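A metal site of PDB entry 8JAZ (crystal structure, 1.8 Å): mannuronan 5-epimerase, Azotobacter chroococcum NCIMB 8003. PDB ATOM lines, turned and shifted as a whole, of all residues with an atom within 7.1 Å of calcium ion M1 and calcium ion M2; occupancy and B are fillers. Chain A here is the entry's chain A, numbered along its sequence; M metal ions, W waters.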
ATOM      1  N   ASN A 322     -24.844  -5.121 -37.120  1.00  0.00           N
ATOM      2  CA  ASN A 322     -26.095  -4.727 -36.462  1.00  0.00           C
ATOM      3  C   ASN A 322     -27.297  -5.496 -37.019  1.00  0.00           C
ATOM      4  O   ASN A 322     -28.228  -4.919 -37.587  1.00  0.00           O
ATOM      5  CB  ASN A 322     -26.304  -3.212 -36.578  1.00  0.00           C
ATOM      6  CG  ASN A 322     -25.121  -2.421 -36.036  1.00  0.00           C
ATOM      7  OD1 ASN A 322     -24.602  -1.523 -36.707  1.00  0.00           O
ATOM      8  ND2 ASN A 322     -24.673  -2.754 -34.828  1.00  0.00           N
ATOM      9  N   SER A 338     -22.272 -12.138 -37.953  1.00  0.00           N
ATOM     10  CA  SER A 338     -22.215 -10.692 -37.805  1.00  0.00           C
ATOM     11  C   SER A 338     -20.881 -10.331 -37.159  1.00  0.00           C
ATOM     12  O   SER A 338     -19.971 -11.154 -37.057  1.00  0.00           O
ATOM     13  CB  SER A 338     -23.415 -10.174 -36.999  1.00  0.00           C
ATOM     14  OG  SER A 338     -23.657  -8.806 -37.276  1.00  0.00           O
ATOM     15  N   SER A 339     -20.774  -9.082 -36.701  1.00  0.00           N
ATOM     16  CA  SER A 339     -19.501  -8.535 -36.243  1.00  0.00           C
ATOM     17  C   SER A 339     -19.781  -7.538 -35.122  1.00  0.00           C
ATOM     18  O   SER A 339     -20.841  -7.601 -34.485  1.00  0.00           O
ATOM     19  CB  SER A 339     -18.736  -7.913 -37.430  1.00  0.00           C
ATOM     20  OG  SER A 339     -17.528  -7.319 -36.996  1.00  0.00           O
ATOM     21  N   GLU A 340     -18.824  -6.648 -34.860  1.00  0.00           N
ATOM     22  CA  GLU A 340     -18.892  -5.706 -33.744  1.00  0.00           C
ATOM     23  C   GLU A 340     -20.272  -5.080 -33.596  1.00  0.00           C
ATOM     24  O   GLU A 340     -20.949  -4.767 -34.581  1.00  0.00           O
ATOM     25  CB  GLU A 340     -17.833  -4.610 -33.908  1.00  0.00           C
ATOM     26  CG  GLU A 340     -17.551  -3.723 -32.677  1.00  0.00           C
ATOM     27  CD  GLU A 340     -17.225  -4.470 -31.378  1.00  0.00           C
ATOM     28  OE1 GLU A 340     -16.184  -4.150 -30.769  1.00  0.00           O
ATOM     29  OE2 GLU A 340     -18.046  -5.299 -30.921  1.00  0.00           O
ATOM     30  N   GLY A 341     -20.678  -4.902 -32.343  1.00  0.00           N
ATOM     31  CA  GLY A 341     -22.021  -4.482 -32.004  1.00  0.00           C
ATOM     32  C   GLY A 341     -22.837  -5.641 -31.448  1.00  0.00           C
ATOM     33  O   GLY A 341     -22.454  -6.813 -31.518  1.00  0.00           O
ATOM     34  N   ARG A 342     -23.977  -5.278 -30.867  1.00  0.00           N
ATOM     35  CA  ARG A 342     -24.888  -6.256 -30.280  1.00  0.00           C
ATOM     36  C   ARG A 342     -25.805  -6.796 -31.371  1.00  0.00           C
ATOM     37  O   ARG A 342     -26.514  -6.023 -32.025  1.00  0.00           O
ATOM     38  CB  ARG A 342     -25.690  -5.631 -29.144  1.00  0.00           C
ATOM     39  CG  ARG A 342     -26.901  -6.443 -28.721  1.00  0.00           C
ATOM     40  CD  ARG A 342     -27.272  -6.152 -27.277  1.00  0.00           C
ATOM     41  NE  ARG A 342     -28.460  -6.880 -26.838  1.00  0.00           N
ATOM     42  CZ  ARG A 342     -28.472  -8.173 -26.542  1.00  0.00           C
ATOM     43  NH1 ARG A 342     -27.386  -8.926 -26.637  1.00  0.00           N
ATOM     44  NH2 ARG A 342     -29.607  -8.732 -26.143  1.00  0.00           N
ATOM     45  N   ASP A 343     -25.790  -8.111 -31.557  1.00  0.00           N
ATOM     46  CA  ASP A 343     -26.584  -8.766 -32.585  1.00  0.00           C
ATOM     47  C   ASP A 343     -27.516  -9.776 -31.939  1.00  0.00           C
ATOM     48  O   ASP A 343     -27.131 -10.496 -31.010  1.00  0.00           O
ATOM     49  CB  ASP A 343     -25.700  -9.482 -33.616  1.00  0.00           C
ATOM     50  CG  ASP A 343     -24.769  -8.524 -34.351  1.00  0.00           C
ATOM     51  OD1 ASP A 343     -25.251  -7.760 -35.218  1.00  0.00           O
ATOM     52  OD2 ASP A 343     -23.549  -8.542 -34.070  1.00  0.00           O
ATOM     53  N   LEU A 344     -28.764  -9.818 -32.408  1.00  0.00           N
ATOM     54  CA  LEU A 344     -29.745 -10.818 -31.996  1.00  0.00           C
ATOM     55  C   LEU A 344     -29.964 -11.760 -33.166  1.00  0.00           C
ATOM     56  O   LEU A 344     -30.541 -11.367 -34.186  1.00  0.00           O
ATOM     57  CB  LEU A 344     -31.054 -10.163 -31.559  1.00  0.00           C
ATOM     58  CG  LEU A 344     -30.934  -8.942 -30.639  1.00  0.00           C
ATOM     59  CD1 LEU A 344     -32.319  -8.392 -30.309  1.00  0.00           C
ATOM     60  CD2 LEU A 344     -30.167  -9.266 -29.378  1.00  0.00           C
ATOM     61  N   LEU A 345     -29.520 -13.008 -33.026  1.00  0.00           N
ATOM     62  CA  LEU A 345     -29.547 -13.988 -34.097  1.00  0.00           C
ATOM     63  C   LEU A 345     -30.341 -15.197 -33.630  1.00  0.00           C
ATOM     64  O   LEU A 345     -29.946 -15.880 -32.669  1.00  0.00           O
ATOM     65  CB  LEU A 345     -28.133 -14.390 -34.508  1.00  0.00           C
ATOM     66  CG  LEU A 345     -27.190 -13.246 -34.879  1.00  0.00           C
ATOM     67  CD1 LEU A 345     -25.855 -13.764 -35.389  1.00  0.00           C
ATOM     68  CD2 LEU A 345     -27.839 -12.337 -35.924  1.00  0.00           C
ATOM     69  N   ASP A 355     -22.847 -17.027 -35.225  1.00  0.00           N
ATOM     70  CA  ASP A 355     -21.657 -16.387 -34.681  1.00  0.00           C
ATOM     71  C   ASP A 355     -21.912 -14.887 -34.697  1.00  0.00           C
ATOM     72  O   ASP A 355     -21.924 -14.271 -35.764  1.00  0.00           O
ATOM     73  CB  ASP A 355     -20.406 -16.744 -35.476  1.00  0.00           C
ATOM     74  CG  ASP A 355     -19.122 -16.258 -34.809  1.00  0.00           C
ATOM     75  OD1 ASP A 355     -19.208 -15.538 -33.792  1.00  0.00           O
ATOM     76  OD2 ASP A 355     -18.032 -16.601 -35.306  1.00  0.00           O
ATOM     77  N   GLY A 356     -22.139 -14.300 -33.521  1.00  0.00           N
ATOM     78  CA  GLY A 356     -22.413 -12.882 -33.447  1.00  0.00           C
ATOM     79  C   GLY A 356     -21.204 -11.981 -33.564  1.00  0.00           C
ATOM     80  O   GLY A 356     -21.364 -10.766 -33.697  1.00  0.00           O
ATOM     81  N   GLY A 357     -19.997 -12.556 -33.544  1.00  0.00           N
ATOM     82  CA  GLY A 357     -18.793 -11.758 -33.633  1.00  0.00           C
ATOM     83  C   GLY A 357     -18.536 -10.980 -32.353  1.00  0.00           C
ATOM     84  O   GLY A 357     -18.949 -11.375 -31.255  1.00  0.00           O
ATOM     85  N   ALA A 358     -17.847  -9.857 -32.502  1.00  0.00           N
ATOM     86  CA  ALA A 358     -17.552  -9.010 -31.361  1.00  0.00           C
ATOM     87  C   ALA A 358     -18.828  -8.386 -30.802  1.00  0.00           C
ATOM     88  O   ALA A 358     -19.861  -8.310 -31.486  1.00  0.00           O
ATOM     89  CB  ALA A 358     -16.548  -7.926 -31.757  1.00  0.00           C
ATOM     90  N   GLY A 359     -18.753  -7.942 -29.556  1.00  0.00           N
ATOM     91  CA  GLY A 359     -19.896  -7.393 -28.873  1.00  0.00           C
ATOM     92  C   GLY A 359     -20.701  -8.458 -28.139  1.00  0.00           C
ATOM     93  O   GLY A 359     -20.438  -9.657 -28.221  1.00  0.00           O
ATOM     94  N   ARG A 360     -21.698  -7.988 -27.396  1.00  0.00           N
ATOM     95  CA  ARG A 360     -22.564  -8.863 -26.603  1.00  0.00           C
ATOM     96  C   ARG A 360     -23.750  -9.280 -27.474  1.00  0.00           C
ATOM     97  O   ARG A 360     -24.579  -8.434 -27.840  1.00  0.00           O
ATOM     98  CB  ARG A 360     -23.018  -8.165 -25.333  1.00  0.00           C
ATOM     99  CG  ARG A 360     -23.881  -9.021 -24.435  1.00  0.00           C
ATOM    100  CD  ARG A 360     -24.208  -8.317 -23.131  1.00  0.00           C
ATOM    101  NE  ARG A 360     -25.212  -7.273 -23.296  1.00  0.00           N
ATOM    102  CZ  ARG A 360     -26.519  -7.500 -23.406  1.00  0.00           C
ATOM    103  NH1 ARG A 360     -27.014  -8.727 -23.365  1.00  0.00           N
ATOM    104  NH2 ARG A 360     -27.341  -6.471 -23.557  1.00  0.00           N
ATOM    105  N   ASP A 361     -23.837 -10.560 -27.802  1.00  0.00           N
ATOM    106  CA  ASP A 361     -24.828 -11.076 -28.724  1.00  0.00           C
ATOM    107  C   ASP A 361     -25.779 -12.043 -28.010  1.00  0.00           C
ATOM    108  O   ASP A 361     -25.407 -12.680 -27.030  1.00  0.00           O
ATOM    109  CB  ASP A 361     -24.170 -11.795 -29.902  1.00  0.00           C
ATOM    110  CG  ASP A 361     -23.087 -10.954 -30.553  1.00  0.00           C
ATOM    111  OD1 ASP A 361     -23.376  -9.825 -30.992  1.00  0.00           O
ATOM    112  OD2 ASP A 361     -21.929 -11.428 -30.625  1.00  0.00           O
ATOM    113  N   THR A 362     -27.003 -12.133 -28.525  1.00  0.00           N
ATOM    114  CA  THR A 362     -28.003 -13.072 -28.046  1.00  0.00           C
ATOM    115  C   THR A 362     -28.309 -14.063 -29.156  1.00  0.00           C
ATOM    116  O   THR A 362     -28.892 -13.694 -30.189  1.00  0.00           O
ATOM    117  CB  THR A 362     -29.276 -12.350 -27.600  1.00  0.00           C
ATOM    118  OG1 THR A 362     -28.960 -11.453 -26.519  1.00  0.00           O
ATOM    119  CG2 THR A 362     -30.331 -13.335 -27.146  1.00  0.00           C
ATOM    120  N   LEU A 363     -27.940 -15.324 -28.965  1.00  0.00           N
ATOM    121  CA  LEU A 363     -28.054 -16.354 -29.990  1.00  0.00           C
ATOM    122  C   LEU A 363     -29.068 -17.407 -29.567  1.00  0.00           C
ATOM    123  O   LEU A 363     -29.141 -17.784 -28.394  1.00  0.00           O
ATOM    124  CB  LEU A 363     -26.693 -17.011 -30.242  1.00  0.00           C
ATOM    125  CG  LEU A 363     -25.468 -16.116 -30.387  1.00  0.00           C
ATOM    126  CD1 LEU A 363     -24.198 -16.936 -30.274  1.00  0.00           C
ATOM    127  CD2 LEU A 363     -25.493 -15.342 -31.691  1.00  0.00           C
ATOM    128  N   PHE A 374     -17.631 -19.399 -31.595  1.00  0.00           N
ATOM    129  CA  PHE A 374     -16.977 -18.269 -30.957  1.00  0.00           C
ATOM    130  C   PHE A 374     -15.535 -18.251 -31.451  1.00  0.00           C
ATOM    131  O   PHE A 374     -14.726 -19.103 -31.063  1.00  0.00           O
ATOM    132  CB  PHE A 374     -17.048 -18.386 -29.432  1.00  0.00           C
ATOM    133  CG  PHE A 374     -18.452 -18.334 -28.886  1.00  0.00           C
ATOM    134  CD1 PHE A 374     -18.953 -17.158 -28.347  1.00  0.00           C
ATOM    135  CD2 PHE A 374     -19.259 -19.454 -28.921  1.00  0.00           C
ATOM    136  CE1 PHE A 374     -20.251 -17.114 -27.858  1.00  0.00           C
ATOM    137  CE2 PHE A 374     -20.557 -19.410 -28.431  1.00  0.00           C
ATOM    138  CZ  PHE A 374     -21.045 -18.233 -27.900  1.00  0.00           C
ATOM    139  N   GLN A 378     -11.908 -12.296 -27.434  1.00  0.00           N
ATOM    140  CA  GLN A 378     -12.435 -10.965 -27.168  1.00  0.00           C
ATOM    141  C   GLN A 378     -13.922 -10.829 -27.490  1.00  0.00           C
ATOM    142  O   GLN A 378     -14.509  -9.799 -27.162  1.00  0.00           O
ATOM    143  CB  GLN A 378     -11.667  -9.925 -27.992  1.00  0.00           C
ATOM    144  CG  GLN A 378     -10.170 -10.169 -28.102  1.00  0.00           C
ATOM    145  CD  GLN A 378      -9.421  -8.953 -28.604  1.00  0.00           C
ATOM    146  OE1 GLN A 378      -8.478  -9.076 -29.390  1.00  0.00           O
ATOM    147  NE2 GLN A 378      -9.859  -7.768 -28.180  1.00  0.00           N
ATOM    148  N   ASP A 379     -14.531 -11.839 -28.115  1.00  0.00           N
ATOM    149  CA  ASP A 379     -15.896 -11.723 -28.621  1.00  0.00           C
ATOM    150  C   ASP A 379     -16.967 -11.963 -27.556  1.00  0.00           C
ATOM    151  O   ASP A 379     -18.148 -11.740 -27.844  1.00  0.00           O
ATOM    152  CB  ASP A 379     -16.105 -12.693 -29.776  1.00  0.00           C
ATOM    153  CG  ASP A 379     -15.400 -12.243 -31.044  1.00  0.00           C
ATOM    154  OD1 ASP A 379     -14.783 -11.160 -31.026  1.00  0.00           O
ATOM    155  OD2 ASP A 379     -15.463 -12.984 -32.052  1.00  0.00           O
ATOM    156  N   SER A 380     -16.596 -12.424 -26.360  1.00  0.00           N
ATOM    157  CA  SER A 380     -17.573 -12.669 -25.302  1.00  0.00           C
ATOM    158  C   SER A 380     -16.827 -12.677 -23.975  1.00  0.00           C
ATOM    159  O   SER A 380     -16.009 -13.567 -23.741  1.00  0.00           O
ATOM    160  CB  SER A 380     -18.316 -13.977 -25.531  1.00  0.00           C
ATOM    161  OG  SER A 380     -19.342 -14.168 -24.582  1.00  0.00           O
ATOM    162  N   PHE A 381     -17.097 -11.696 -23.115  1.00  0.00           N
ATOM    163  CA  PHE A 381     -16.301 -11.569 -21.904  1.00  0.00           C
ATOM    164  C   PHE A 381     -17.056 -10.817 -20.819  1.00  0.00           C
ATOM    165  O   PHE A 381     -18.025 -10.107 -21.083  1.00  0.00           O
ATOM    166  CB  PHE A 381     -14.952 -10.884 -22.199  1.00  0.00           C
ATOM    167  CG  PHE A 381     -15.086  -9.453 -22.623  1.00  0.00           C
ATOM    168  CD1 PHE A 381     -15.051  -8.429 -21.690  1.00  0.00           C
ATOM    169  CD2 PHE A 381     -15.216  -9.124 -23.961  1.00  0.00           C
ATOM    170  CE1 PHE A 381     -15.173  -7.105 -22.085  1.00  0.00           C
ATOM    171  CE2 PHE A 381     -15.333  -7.806 -24.363  1.00  0.00           C
ATOM    172  CZ  PHE A 381     -15.314  -6.794 -23.415  1.00  0.00           C
ATOM    173  N   ARG A 390     -20.279  -8.357 -21.071  1.00  0.00           N
ATOM    174  CA  ARG A 390     -20.303  -8.387 -22.528  1.00  0.00           C
ATOM    175  C   ARG A 390     -20.318  -9.842 -22.952  1.00  0.00           C
ATOM    176  O   ARG A 390     -19.567 -10.275 -23.845  1.00  0.00           O
ATOM    177  CB  ARG A 390     -19.078  -7.682 -23.101  1.00  0.00           C
ATOM    178  CG  ARG A 390     -18.773  -6.317 -22.482  1.00  0.00           C
ATOM    179  CD  ARG A 390     -19.781  -5.253 -22.889  1.00  0.00           C
ATOM    180  NE  ARG A 390     -20.247  -5.448 -24.254  1.00  0.00           N
ATOM    181  CZ  ARG A 390     -20.080  -4.553 -25.227  1.00  0.00           C
ATOM    182  NH1 ARG A 390     -19.444  -3.417 -25.022  1.00  0.00           N
ATOM    183  NH2 ARG A 390     -20.568  -4.821 -26.439  1.00  0.00           N
ATOM    184  N   VAL A 391     -21.142 -10.633 -22.264  1.00  0.00           N
ATOM    185  CA  VAL A 391     -21.166 -12.087 -22.397  1.00  0.00           C
ATOM    186  C   VAL A 391     -22.284 -12.482 -23.348  1.00  0.00           C
ATOM    187  O   VAL A 391     -23.468 -12.183 -23.095  1.00  0.00           O
ATOM    188  CB  VAL A 391     -21.347 -12.762 -21.035  1.00  0.00           C
ATOM    189  CG1 VAL A 391     -21.581 -14.262 -21.206  1.00  0.00           C
ATOM    190  CG2 VAL A 391     -20.147 -12.505 -20.147  1.00  0.00           C
ATOM    191  N   ASP A 392     -21.921 -13.135 -24.450  1.00  0.00           N
ATOM    192  CA  ASP A 392     -22.932 -13.702 -25.326  1.00  0.00           C
ATOM    193  C   ASP A 392     -23.738 -14.750 -24.579  1.00  0.00           C
ATOM    194  O   ASP A 392     -23.187 -15.594 -23.864  1.00  0.00           O
ATOM    195  CB  ASP A 392     -22.269 -14.337 -26.559  1.00  0.00           C
ATOM    196  CG  ASP A 392     -21.772 -13.310 -27.551  1.00  0.00           C
ATOM    197  OD1 ASP A 392     -21.758 -12.098 -27.210  1.00  0.00           O
ATOM    198  OD2 ASP A 392     -21.386 -13.707 -28.669  1.00  0.00           O
HETATM  199 CA    CA M   1     -20.188 -11.904 -29.184  1.00  0.00          CA
HETATM  200 CA    CA M   2     -21.829  -8.811 -32.543  1.00  0.00          CA
HETATM  201  O   HOH W   1     -19.296 -14.022 -30.182  1.00  0.00           O
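The side-chain hydroxyl of Ser 380 lies within hydrogen-bond range of the backbone NH of Asp 392 (2.8 Å). The side-chain hydroxyl (OG) of Ser 338 is in hydrogen-bond range of the side-chain carboxylate (OD1) of Asp 343. N of Asn 322 sits at hydrogen-bond distance from OD1 of Asp 343 (3.3 Å). N of Thr 362 is in hydrogen-bond range of O of Asp 343, 3.0 Å away. The backbone NH of Gly 359 lies within hydrogen-bond range of the side-chain carboxylate of Glu 340, at 3.1 Å. The backbone NH (N) of Gly 357 lies within hydrogen-bond range of the side-chain carboxylate (OD1) of Asp 355, 3.1 Å away.
Within 4 Å of calcium ion M1: Gly 357, Gly 359, Asp 361, Asp 379 and Asp 392. The nearest printed residue that does not touch calcium ion M1 is Ala 358 (4.1 Å).
Within 4 Å of calcium ion M2: Ser 339, Gly 341, Asp 343, Gly 356, Gly 357, Ala 358 and Asp 361. The nearest printed residue that does not touch calcium ion M2 is Glu 340 (4.2 Å).
Calcium ion M1 is bound by the side-chain carboxylate (OD2) of Asp 392 (2.2 Å), the side-chain carboxylate (OD2) of Asp 361 (2.3 Å), the backbone carbonyl oxygen (O) of Asp 379 (2.4 Å), the backbone carbonyl oxygen (O) of Gly 359 (2.5 Å), the backbone carbonyl oxygen (O) of Gly 357 (2.5 Å), water W1 (2.5 Å) and the side-chain carboxylate (OD1) of Asp 392 (2.5 Å).
O of Ala 358 binds calcium ion M2 (2.3 Å). The side-chain carboxylate (OD2) of Asp 343 is bound to calcium ion M2, at 2.3 Å. O of Gly 356 binds calcium ion M2 (2.3 Å). O of Gly 341 binds calcium ion M2. The side-chain carboxylate (OD1) of Asp 361 binds calcium ion M2 (2.4 Å). O of Ser 339 is bound to calcium ion M2, 2.5 Å away. Calcium ion M2 has six donor atoms within binding distance.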
